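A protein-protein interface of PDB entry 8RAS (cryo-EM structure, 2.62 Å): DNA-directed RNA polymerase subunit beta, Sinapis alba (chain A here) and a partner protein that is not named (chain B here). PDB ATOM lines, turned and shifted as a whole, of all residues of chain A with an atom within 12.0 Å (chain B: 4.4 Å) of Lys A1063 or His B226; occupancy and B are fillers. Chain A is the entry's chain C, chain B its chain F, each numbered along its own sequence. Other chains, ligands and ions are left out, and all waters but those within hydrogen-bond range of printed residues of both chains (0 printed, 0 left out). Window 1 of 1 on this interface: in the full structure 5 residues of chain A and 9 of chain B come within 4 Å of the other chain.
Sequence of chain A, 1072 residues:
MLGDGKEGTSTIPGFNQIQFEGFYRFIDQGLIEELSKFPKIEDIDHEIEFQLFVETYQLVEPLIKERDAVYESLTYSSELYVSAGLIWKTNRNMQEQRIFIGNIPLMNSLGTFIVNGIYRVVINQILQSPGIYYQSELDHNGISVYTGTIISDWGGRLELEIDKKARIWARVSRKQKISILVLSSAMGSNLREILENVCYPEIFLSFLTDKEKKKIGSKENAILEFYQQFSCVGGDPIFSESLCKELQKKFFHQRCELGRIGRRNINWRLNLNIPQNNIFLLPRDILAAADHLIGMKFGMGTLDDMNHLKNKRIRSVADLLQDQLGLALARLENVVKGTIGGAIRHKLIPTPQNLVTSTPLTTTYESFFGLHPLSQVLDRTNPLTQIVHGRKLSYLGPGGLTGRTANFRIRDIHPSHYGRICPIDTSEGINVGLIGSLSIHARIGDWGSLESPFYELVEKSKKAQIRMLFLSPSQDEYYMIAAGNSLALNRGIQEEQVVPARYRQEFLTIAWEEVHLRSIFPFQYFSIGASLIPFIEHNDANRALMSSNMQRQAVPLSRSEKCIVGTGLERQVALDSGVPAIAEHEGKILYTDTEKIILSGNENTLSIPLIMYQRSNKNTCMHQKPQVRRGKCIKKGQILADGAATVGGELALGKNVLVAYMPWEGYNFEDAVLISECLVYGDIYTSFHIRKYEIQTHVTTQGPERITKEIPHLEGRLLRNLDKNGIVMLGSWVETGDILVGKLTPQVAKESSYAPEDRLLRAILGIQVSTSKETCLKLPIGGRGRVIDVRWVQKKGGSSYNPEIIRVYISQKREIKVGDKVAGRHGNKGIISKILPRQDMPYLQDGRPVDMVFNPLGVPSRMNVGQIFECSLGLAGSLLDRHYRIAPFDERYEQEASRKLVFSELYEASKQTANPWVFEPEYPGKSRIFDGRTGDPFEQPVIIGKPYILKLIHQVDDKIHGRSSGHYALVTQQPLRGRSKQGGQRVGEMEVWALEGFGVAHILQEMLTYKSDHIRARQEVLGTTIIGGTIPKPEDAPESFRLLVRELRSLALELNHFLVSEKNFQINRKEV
A ring nitrogen (ND1) of His B226 lies within hydrogen-bond range of the backbone carbonyl oxygen (O) of Lys A1063, 2.8 Å away. The side-chain amino group (NZ) of Lys A1063 sits close to the side-chain carboxylate (OD1) of Asp B231, at 2.3 Å. The backbone carbonyl oxygen (O) of Glu A1062 sits close to a ring nitrogen (ND1) of His B226 (3.2 Å). The side-chain hydroxyl of Ser B227 is in hydrogen-bond range of the backbone carbonyl oxygen of Lys A1063.
The backbone NH (N) of Lys A1063 sits close to the side-chain hydroxyl (OG) of Ser A1061. A ring nitrogen (NE2) of His B226 sits at hydrogen-bond distance from the side-chain amide nitrogen of Gln B255 (3.0 Å). OD1 of Asn A1064 sits close to N of Gln A1066 (3.2 Å).
Among the printed residues, merely in contact across the chains: Glu A1062 with Leu B230 (3.3 Å), Phe A1065 with His B226 (3.4 Å), Phe A1065 with Gln B255 (3.5 Å), Asn A1064 with Ser B227 (3.8 Å) and Phe A1065 with Val B254 (3.9 Å).
Of the printed residues of chain B, Glu A1062 touches His B226 and Leu B230. Printed residues of chain B within 4 Å of Lys A1063: His B226 (2.8 Å), Ser B227 (3.4 Å) and Asp B231 (2.3 Å). Printed residues of chain B within 4 Å of Asn A1064: Ser B227. Of the printed residues of chain B, Phe A1065 touches His B226, Val B254 and Gln B255. No residue of chain A comes within 4 Å of Gly B224. Of chain A, only Lys A1063 (3.4 Å) and Asn A1064 (3.8 Å) come within 4 Å of Ser B227. No residue of chain A comes within 4 Å of Asn B228. Of the printed residues of chain A, Leu B230 touches Glu A1062. No residue of chain A comes within 4 Å of Leu B251. Of the printed residues of chain A, Val B254 touches Phe A1065 (3.9 Å). The nearest residue of chain A that does not touch His B226 is Asn A1064 (4.8 Å). The nearest printed residue of chain B that does not touch Asn A1064 is His B226 (4.8 Å).
Of the 11 printed residues of chain B, 6 touch a printed residue of chain A. Of the 10 printed residues of chain A, 4 touch a printed residue of chain B. Hydrophobic or aromatic side chains of chain A within 4 Å of the printed part of chain B: Phe A1065. Among the printed residues, Asp or Glu carboxylates within 4 Å of a Lys or Arg side-chain nitrogen of the other chain: Lys A1063 with Asp B231 (2.3 Å).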
ATOM      1  N   LEU A1059      -1.780  15.840 -13.788  1.00  0.00           N
ATOM      2  CA  LEU A1059      -3.028  15.368 -14.367  1.00  0.00           C
ATOM      3  C   LEU A1059      -4.098  15.352 -13.289  1.00  0.00           C
ATOM      4  O   LEU A1059      -3.917  14.726 -12.240  1.00  0.00           O
ATOM      5  CB  LEU A1059      -2.870  13.969 -14.967  1.00  0.00           C
ATOM      6  CG  LEU A1059      -2.028  13.803 -16.233  1.00  0.00           C
ATOM      7  CD1 LEU A1059      -2.584  12.676 -17.083  1.00  0.00           C
ATOM      8  CD2 LEU A1059      -1.966  15.093 -17.029  1.00  0.00           C
ATOM      9  N   VAL A1060      -5.206  16.038 -13.545  1.00  0.00           N
ATOM     10  CA  VAL A1060      -6.335  16.078 -12.626  1.00  0.00           C
ATOM     11  C   VAL A1060      -7.410  15.152 -13.169  1.00  0.00           C
ATOM     12  O   VAL A1060      -7.918  15.358 -14.278  1.00  0.00           O
ATOM     13  CB  VAL A1060      -6.869  17.508 -12.452  1.00  0.00           C
ATOM     14  CG1 VAL A1060      -8.055  17.517 -11.503  1.00  0.00           C
ATOM     15  CG2 VAL A1060      -5.768  18.424 -11.945  1.00  0.00           C
ATOM     16  N   SER A1061      -7.752  14.125 -12.397  1.00  0.00           N
ATOM     17  CA  SER A1061      -8.756  13.167 -12.834  1.00  0.00           C
ATOM     18  C   SER A1061     -10.117  13.839 -12.923  1.00  0.00           C
ATOM     19  O   SER A1061     -10.518  14.579 -12.020  1.00  0.00           O
ATOM     20  CB  SER A1061      -8.811  11.983 -11.872  1.00  0.00           C
ATOM     21  OG  SER A1061      -9.685  10.979 -12.352  1.00  0.00           O
ATOM     22  N   GLU A1062     -10.827  13.591 -14.020  1.00  0.00           N
ATOM     23  CA  GLU A1062     -12.186  14.096 -14.152  1.00  0.00           C
ATOM     24  C   GLU A1062     -13.195  13.245 -13.398  1.00  0.00           C
ATOM     25  O   GLU A1062     -14.371  13.615 -13.336  1.00  0.00           O
ATOM     26  CB  GLU A1062     -12.575  14.185 -15.631  1.00  0.00           C
ATOM     27  CG  GLU A1062     -12.874  12.850 -16.285  1.00  0.00           C
ATOM     28  CD  GLU A1062     -11.628  12.169 -16.814  1.00  0.00           C
ATOM     29  OE1 GLU A1062     -10.519  12.691 -16.582  1.00  0.00           O
ATOM     30  OE2 GLU A1062     -11.759  11.110 -17.461  1.00  0.00           O
ATOM     31  N   LYS A1063     -12.761  12.126 -12.820  1.00  0.00           N
ATOM     32  CA  LYS A1063     -13.649  11.239 -12.078  1.00  0.00           C
ATOM     33  C   LYS A1063     -13.677  11.589 -10.592  1.00  0.00           C
ATOM     34  O   LYS A1063     -14.737  11.898 -10.041  1.00  0.00           O
ATOM     35  CB  LYS A1063     -13.215   9.784 -12.282  1.00  0.00           C
ATOM     36  CG  LYS A1063     -12.669   9.494 -13.670  1.00  0.00           C
ATOM     37  CD  LYS A1063     -13.569   8.550 -14.446  1.00  0.00           C
ATOM     38  CE  LYS A1063     -14.835   9.250 -14.908  1.00  0.00           C
ATOM     39  NZ  LYS A1063     -15.510   8.499 -16.001  1.00  0.00           N
ATOM     40  N   ASN A1064     -12.518  11.548  -9.935  1.00  0.00           N
ATOM     41  CA  ASN A1064     -12.427  11.796  -8.501  1.00  0.00           C
ATOM     42  C   ASN A1064     -11.552  12.994  -8.156  1.00  0.00           C
ATOM     43  O   ASN A1064     -11.283  13.227  -6.970  1.00  0.00           O
ATOM     44  CB  ASN A1064     -11.912  10.547  -7.779  1.00  0.00           C
ATOM     45  CG  ASN A1064     -10.675   9.967  -8.430  1.00  0.00           C
ATOM     46  OD1 ASN A1064      -9.704  10.675  -8.685  1.00  0.00           O
ATOM     47  ND2 ASN A1064     -10.704   8.669  -8.699  1.00  0.00           N
ATOM     48  N   PHE A1065     -11.098  13.755  -9.153  1.00  0.00           N
ATOM     49  CA  PHE A1065     -10.332  14.986  -8.942  1.00  0.00           C
ATOM     50  C   PHE A1065      -9.040  14.738  -8.168  1.00  0.00           C
ATOM     51  O   PHE A1065      -8.620  15.569  -7.360  1.00  0.00           O
ATOM     52  CB  PHE A1065     -11.177  16.055  -8.245  1.00  0.00           C
ATOM     53  CG  PHE A1065     -12.634  15.995  -8.595  1.00  0.00           C
ATOM     54  CD1 PHE A1065     -13.054  16.192  -9.897  1.00  0.00           C
ATOM     55  CD2 PHE A1065     -13.582  15.726  -7.625  1.00  0.00           C
ATOM     56  CE1 PHE A1065     -14.388  16.132 -10.221  1.00  0.00           C
ATOM     57  CE2 PHE A1065     -14.918  15.665  -7.945  1.00  0.00           C
ATOM     58  CZ  PHE A1065     -15.322  15.869  -9.245  1.00  0.00           C
ATOM     59  N   GLN A1066      -8.397  13.600  -8.411  1.00  0.00           N
ATOM     60  CA  GLN A1066      -7.099  13.306  -7.822  1.00  0.00           C
ATOM     61  C   GLN A1066      -6.000  13.849  -8.724  1.00  0.00           C
ATOM     62  O   GLN A1066      -6.026  13.639  -9.941  1.00  0.00           O
ATOM     63  CB  GLN A1066      -6.921  11.803  -7.612  1.00  0.00           C
ATOM     64  CG  GLN A1066      -5.684  11.435  -6.812  1.00  0.00           C
ATOM     65  CD  GLN A1066      -5.049  10.147  -7.291  1.00  0.00           C
ATOM     66  OE1 GLN A1066      -3.986  10.158  -7.910  1.00  0.00           O
ATOM     67  NE2 GLN A1066      -5.701   9.025  -7.007  1.00  0.00           N
ATOM     68  N   ILE A1067      -5.037  14.543  -8.128  1.00  0.00           N
ATOM     69  CA  ILE A1067      -3.947  15.161  -8.871  1.00  0.00           C
ATOM     70  C   ILE A1067      -2.821  14.145  -9.013  1.00  0.00           C
ATOM     71  O   ILE A1067      -2.318  13.618  -8.017  1.00  0.00           O
ATOM     72  CB  ILE A1067      -3.456  16.440  -8.177  1.00  0.00           C
ATOM     73  CG1 ILE A1067      -4.625  17.397  -7.948  1.00  0.00           C
ATOM     74  CG2 ILE A1067      -2.380  17.116  -9.005  1.00  0.00           C
ATOM     75  CD1 ILE A1067      -4.248  18.643  -7.183  1.00  0.00           C
ATOM     76  N   ASN A1068      -2.427  13.873 -10.253  1.00  0.00           N
ATOM     77  CA  ASN A1068      -1.393  12.897 -10.564  1.00  0.00           C
ATOM     78  C   ASN A1068      -0.183  13.631 -11.125  1.00  0.00           C
ATOM     79  O   ASN A1068      -0.302  14.377 -12.100  1.00  0.00           O
ATOM     80  CB  ASN A1068      -1.914  11.864 -11.569  1.00  0.00           C
ATOM     81  CG  ASN A1068      -0.828  10.931 -12.084  1.00  0.00           C
ATOM     82  OD1 ASN A1068      -0.945  10.377 -13.177  1.00  0.00           O
ATOM     83  ND2 ASN A1068       0.204  10.710 -11.278  1.00  0.00           N
ATOM     84  N   GLY B 224     -21.430  11.559  -2.849  1.00  0.00           N
ATOM     85  CA  GLY B 224     -20.119  12.080  -3.171  1.00  0.00           C
ATOM     86  C   GLY B 224     -19.338  11.259  -4.168  1.00  0.00           C
ATOM     87  O   GLY B 224     -18.128  11.472  -4.309  1.00  0.00           O
ATOM     88  N   ASP B 225     -19.987  10.328  -4.863  1.00  0.00           N
ATOM     89  CA  ASP B 225     -19.321   9.456  -5.830  1.00  0.00           C
ATOM     90  C   ASP B 225     -19.459  10.084  -7.209  1.00  0.00           C
ATOM     91  O   ASP B 225     -20.422   9.839  -7.935  1.00  0.00           O
ATOM     92  CB  ASP B 225     -19.913   8.055  -5.783  1.00  0.00           C
ATOM     93  CG  ASP B 225     -19.081   7.046  -6.544  1.00  0.00           C
ATOM     94  OD1 ASP B 225     -17.967   7.397  -6.983  1.00  0.00           O
ATOM     95  OD2 ASP B 225     -19.540   5.896  -6.700  1.00  0.00           O
ATOM     96  N   HIS B 226     -18.481  10.911  -7.573  1.00  0.00           N
ATOM     97  CA  HIS B 226     -18.514  11.568  -8.873  1.00  0.00           C
ATOM     98  C   HIS B 226     -18.121  10.632 -10.008  1.00  0.00           C
ATOM     99  O   HIS B 226     -18.594  10.808 -11.134  1.00  0.00           O
ATOM    100  CB  HIS B 226     -17.598  12.791  -8.869  1.00  0.00           C
ATOM    101  CG  HIS B 226     -17.671  13.597 -10.127  1.00  0.00           C
ATOM    102  ND1 HIS B 226     -16.779  13.439 -11.165  1.00  0.00           N
ATOM    103  CD2 HIS B 226     -18.534  14.564 -10.518  1.00  0.00           C
ATOM    104  CE1 HIS B 226     -17.088  14.274 -12.139  1.00  0.00           C
ATOM    105  NE2 HIS B 226     -18.149  14.968 -11.772  1.00  0.00           N
ATOM    106  N   SER B 227     -17.260   9.647  -9.742  1.00  0.00           N
ATOM    107  CA  SER B 227     -16.798   8.759 -10.805  1.00  0.00           C
ATOM    108  C   SER B 227     -17.947   7.945 -11.384  1.00  0.00           C
ATOM    109  O   SER B 227     -18.147   7.910 -12.606  1.00  0.00           O
ATOM    110  CB  SER B 227     -15.703   7.837 -10.270  1.00  0.00           C
ATOM    111  OG  SER B 227     -14.774   8.559  -9.482  1.00  0.00           O
ATOM    112  N   ASN B 228     -18.718   7.284 -10.518  1.00  0.00           N
ATOM    113  CA  ASN B 228     -19.836   6.476 -10.989  1.00  0.00           C
ATOM    114  C   ASN B 228     -20.902   7.339 -11.648  1.00  0.00           C
ATOM    115  O   ASN B 228     -21.490   6.944 -12.659  1.00  0.00           O
ATOM    116  CB  ASN B 228     -20.432   5.677  -9.832  1.00  0.00           C
ATOM    117  CG  ASN B 228     -19.576   4.493  -9.441  1.00  0.00           C
ATOM    118  OD1 ASN B 228     -18.813   3.969 -10.251  1.00  0.00           O
ATOM    119  ND2 ASN B 228     -19.698   4.062  -8.193  1.00  0.00           N
ATOM    120  N   ALA B 229     -21.169   8.519 -11.085  1.00  0.00           N
ATOM    121  CA  ALA B 229     -22.163   9.410 -11.674  1.00  0.00           C
ATOM    122  C   ALA B 229     -21.745   9.864 -13.067  1.00  0.00           C
ATOM    123  O   ALA B 229     -22.563   9.887 -13.991  1.00  0.00           O
ATOM    124  CB  ALA B 229     -22.395  10.612 -10.762  1.00  0.00           C
ATOM    125  N   LEU B 230     -20.472  10.228 -13.238  1.00  0.00           N
ATOM    126  CA  LEU B 230     -19.992  10.638 -14.553  1.00  0.00           C
ATOM    127  C   LEU B 230     -20.038   9.483 -15.544  1.00  0.00           C
ATOM    128  O   LEU B 230     -20.417   9.672 -16.707  1.00  0.00           O
ATOM    129  CB  LEU B 230     -18.576  11.200 -14.445  1.00  0.00           C
ATOM    130  CG  LEU B 230     -18.074  11.977 -15.663  1.00  0.00           C
ATOM    131  CD1 LEU B 230     -19.141  12.931 -16.169  1.00  0.00           C
ATOM    132  CD2 LEU B 230     -16.799  12.727 -15.336  1.00  0.00           C
ATOM    133  N   ASP B 231     -19.661   8.280 -15.105  1.00  0.00           N
ATOM    134  CA  ASP B 231     -19.728   7.122 -15.992  1.00  0.00           C
ATOM    135  C   ASP B 231     -21.163   6.839 -16.420  1.00  0.00           C
ATOM    136  O   ASP B 231     -21.428   6.566 -17.598  1.00  0.00           O
ATOM    137  CB  ASP B 231     -19.126   5.899 -15.304  1.00  0.00           C
ATOM    138  CG  ASP B 231     -17.649   5.739 -15.590  1.00  0.00           C
ATOM    139  OD1 ASP B 231     -16.913   6.743 -15.503  1.00  0.00           O
ATOM    140  OD2 ASP B 231     -17.223   4.608 -15.904  1.00  0.00           O
ATOM    141  N   LEU B 251     -23.870  16.722 -11.016  1.00  0.00           N
ATOM    142  CA  LEU B 251     -22.426  16.575 -11.165  1.00  0.00           C
ATOM    143  C   LEU B 251     -21.679  17.737 -10.521  1.00  0.00           C
ATOM    144  O   LEU B 251     -20.647  17.539  -9.872  1.00  0.00           O
ATOM    145  CB  LEU B 251     -22.061  16.462 -12.645  1.00  0.00           C
ATOM    146  CG  LEU B 251     -22.282  15.108 -13.317  1.00  0.00           C
ATOM    147  CD1 LEU B 251     -21.722  15.125 -14.725  1.00  0.00           C
ATOM    148  CD2 LEU B 251     -21.649  13.996 -12.503  1.00  0.00           C
ATOM    149  N   VAL B 254     -20.627  18.015  -6.683  1.00  0.00           N
ATOM    150  CA  VAL B 254     -19.450  17.334  -6.154  1.00  0.00           C
ATOM    151  C   VAL B 254     -18.187  18.040  -6.632  1.00  0.00           C
ATOM    152  O   VAL B 254     -17.184  18.095  -5.912  1.00  0.00           O
ATOM    153  CB  VAL B 254     -19.440  15.850  -6.561  1.00  0.00           C
ATOM    154  CG1 VAL B 254     -18.343  15.107  -5.827  1.00  0.00           C
ATOM    155  CG2 VAL B 254     -20.791  15.218  -6.284  1.00  0.00           C
ATOM    156  N   GLN B 255     -18.224  18.585  -7.851  1.00  0.00           N
ATOM    157  CA  GLN B 255     -17.058  19.285  -8.380  1.00  0.00           C
ATOM    158  C   GLN B 255     -16.774  20.571  -7.615  1.00  0.00           C
ATOM    159  O   GLN B 255     -15.617  20.997  -7.534  1.00  0.00           O
ATOM    160  CB  GLN B 255     -17.248  19.599  -9.863  1.00  0.00           C
ATOM    161  CG  GLN B 255     -17.231  18.392 -10.776  1.00  0.00           C
ATOM    162  CD  GLN B 255     -17.778  18.705 -12.151  1.00  0.00           C
ATOM    163  OE1 GLN B 255     -18.044  19.861 -12.473  1.00  0.00           O
ATOM    164  NE2 GLN B 255     -17.946  17.677 -12.970  1.00  0.00           N
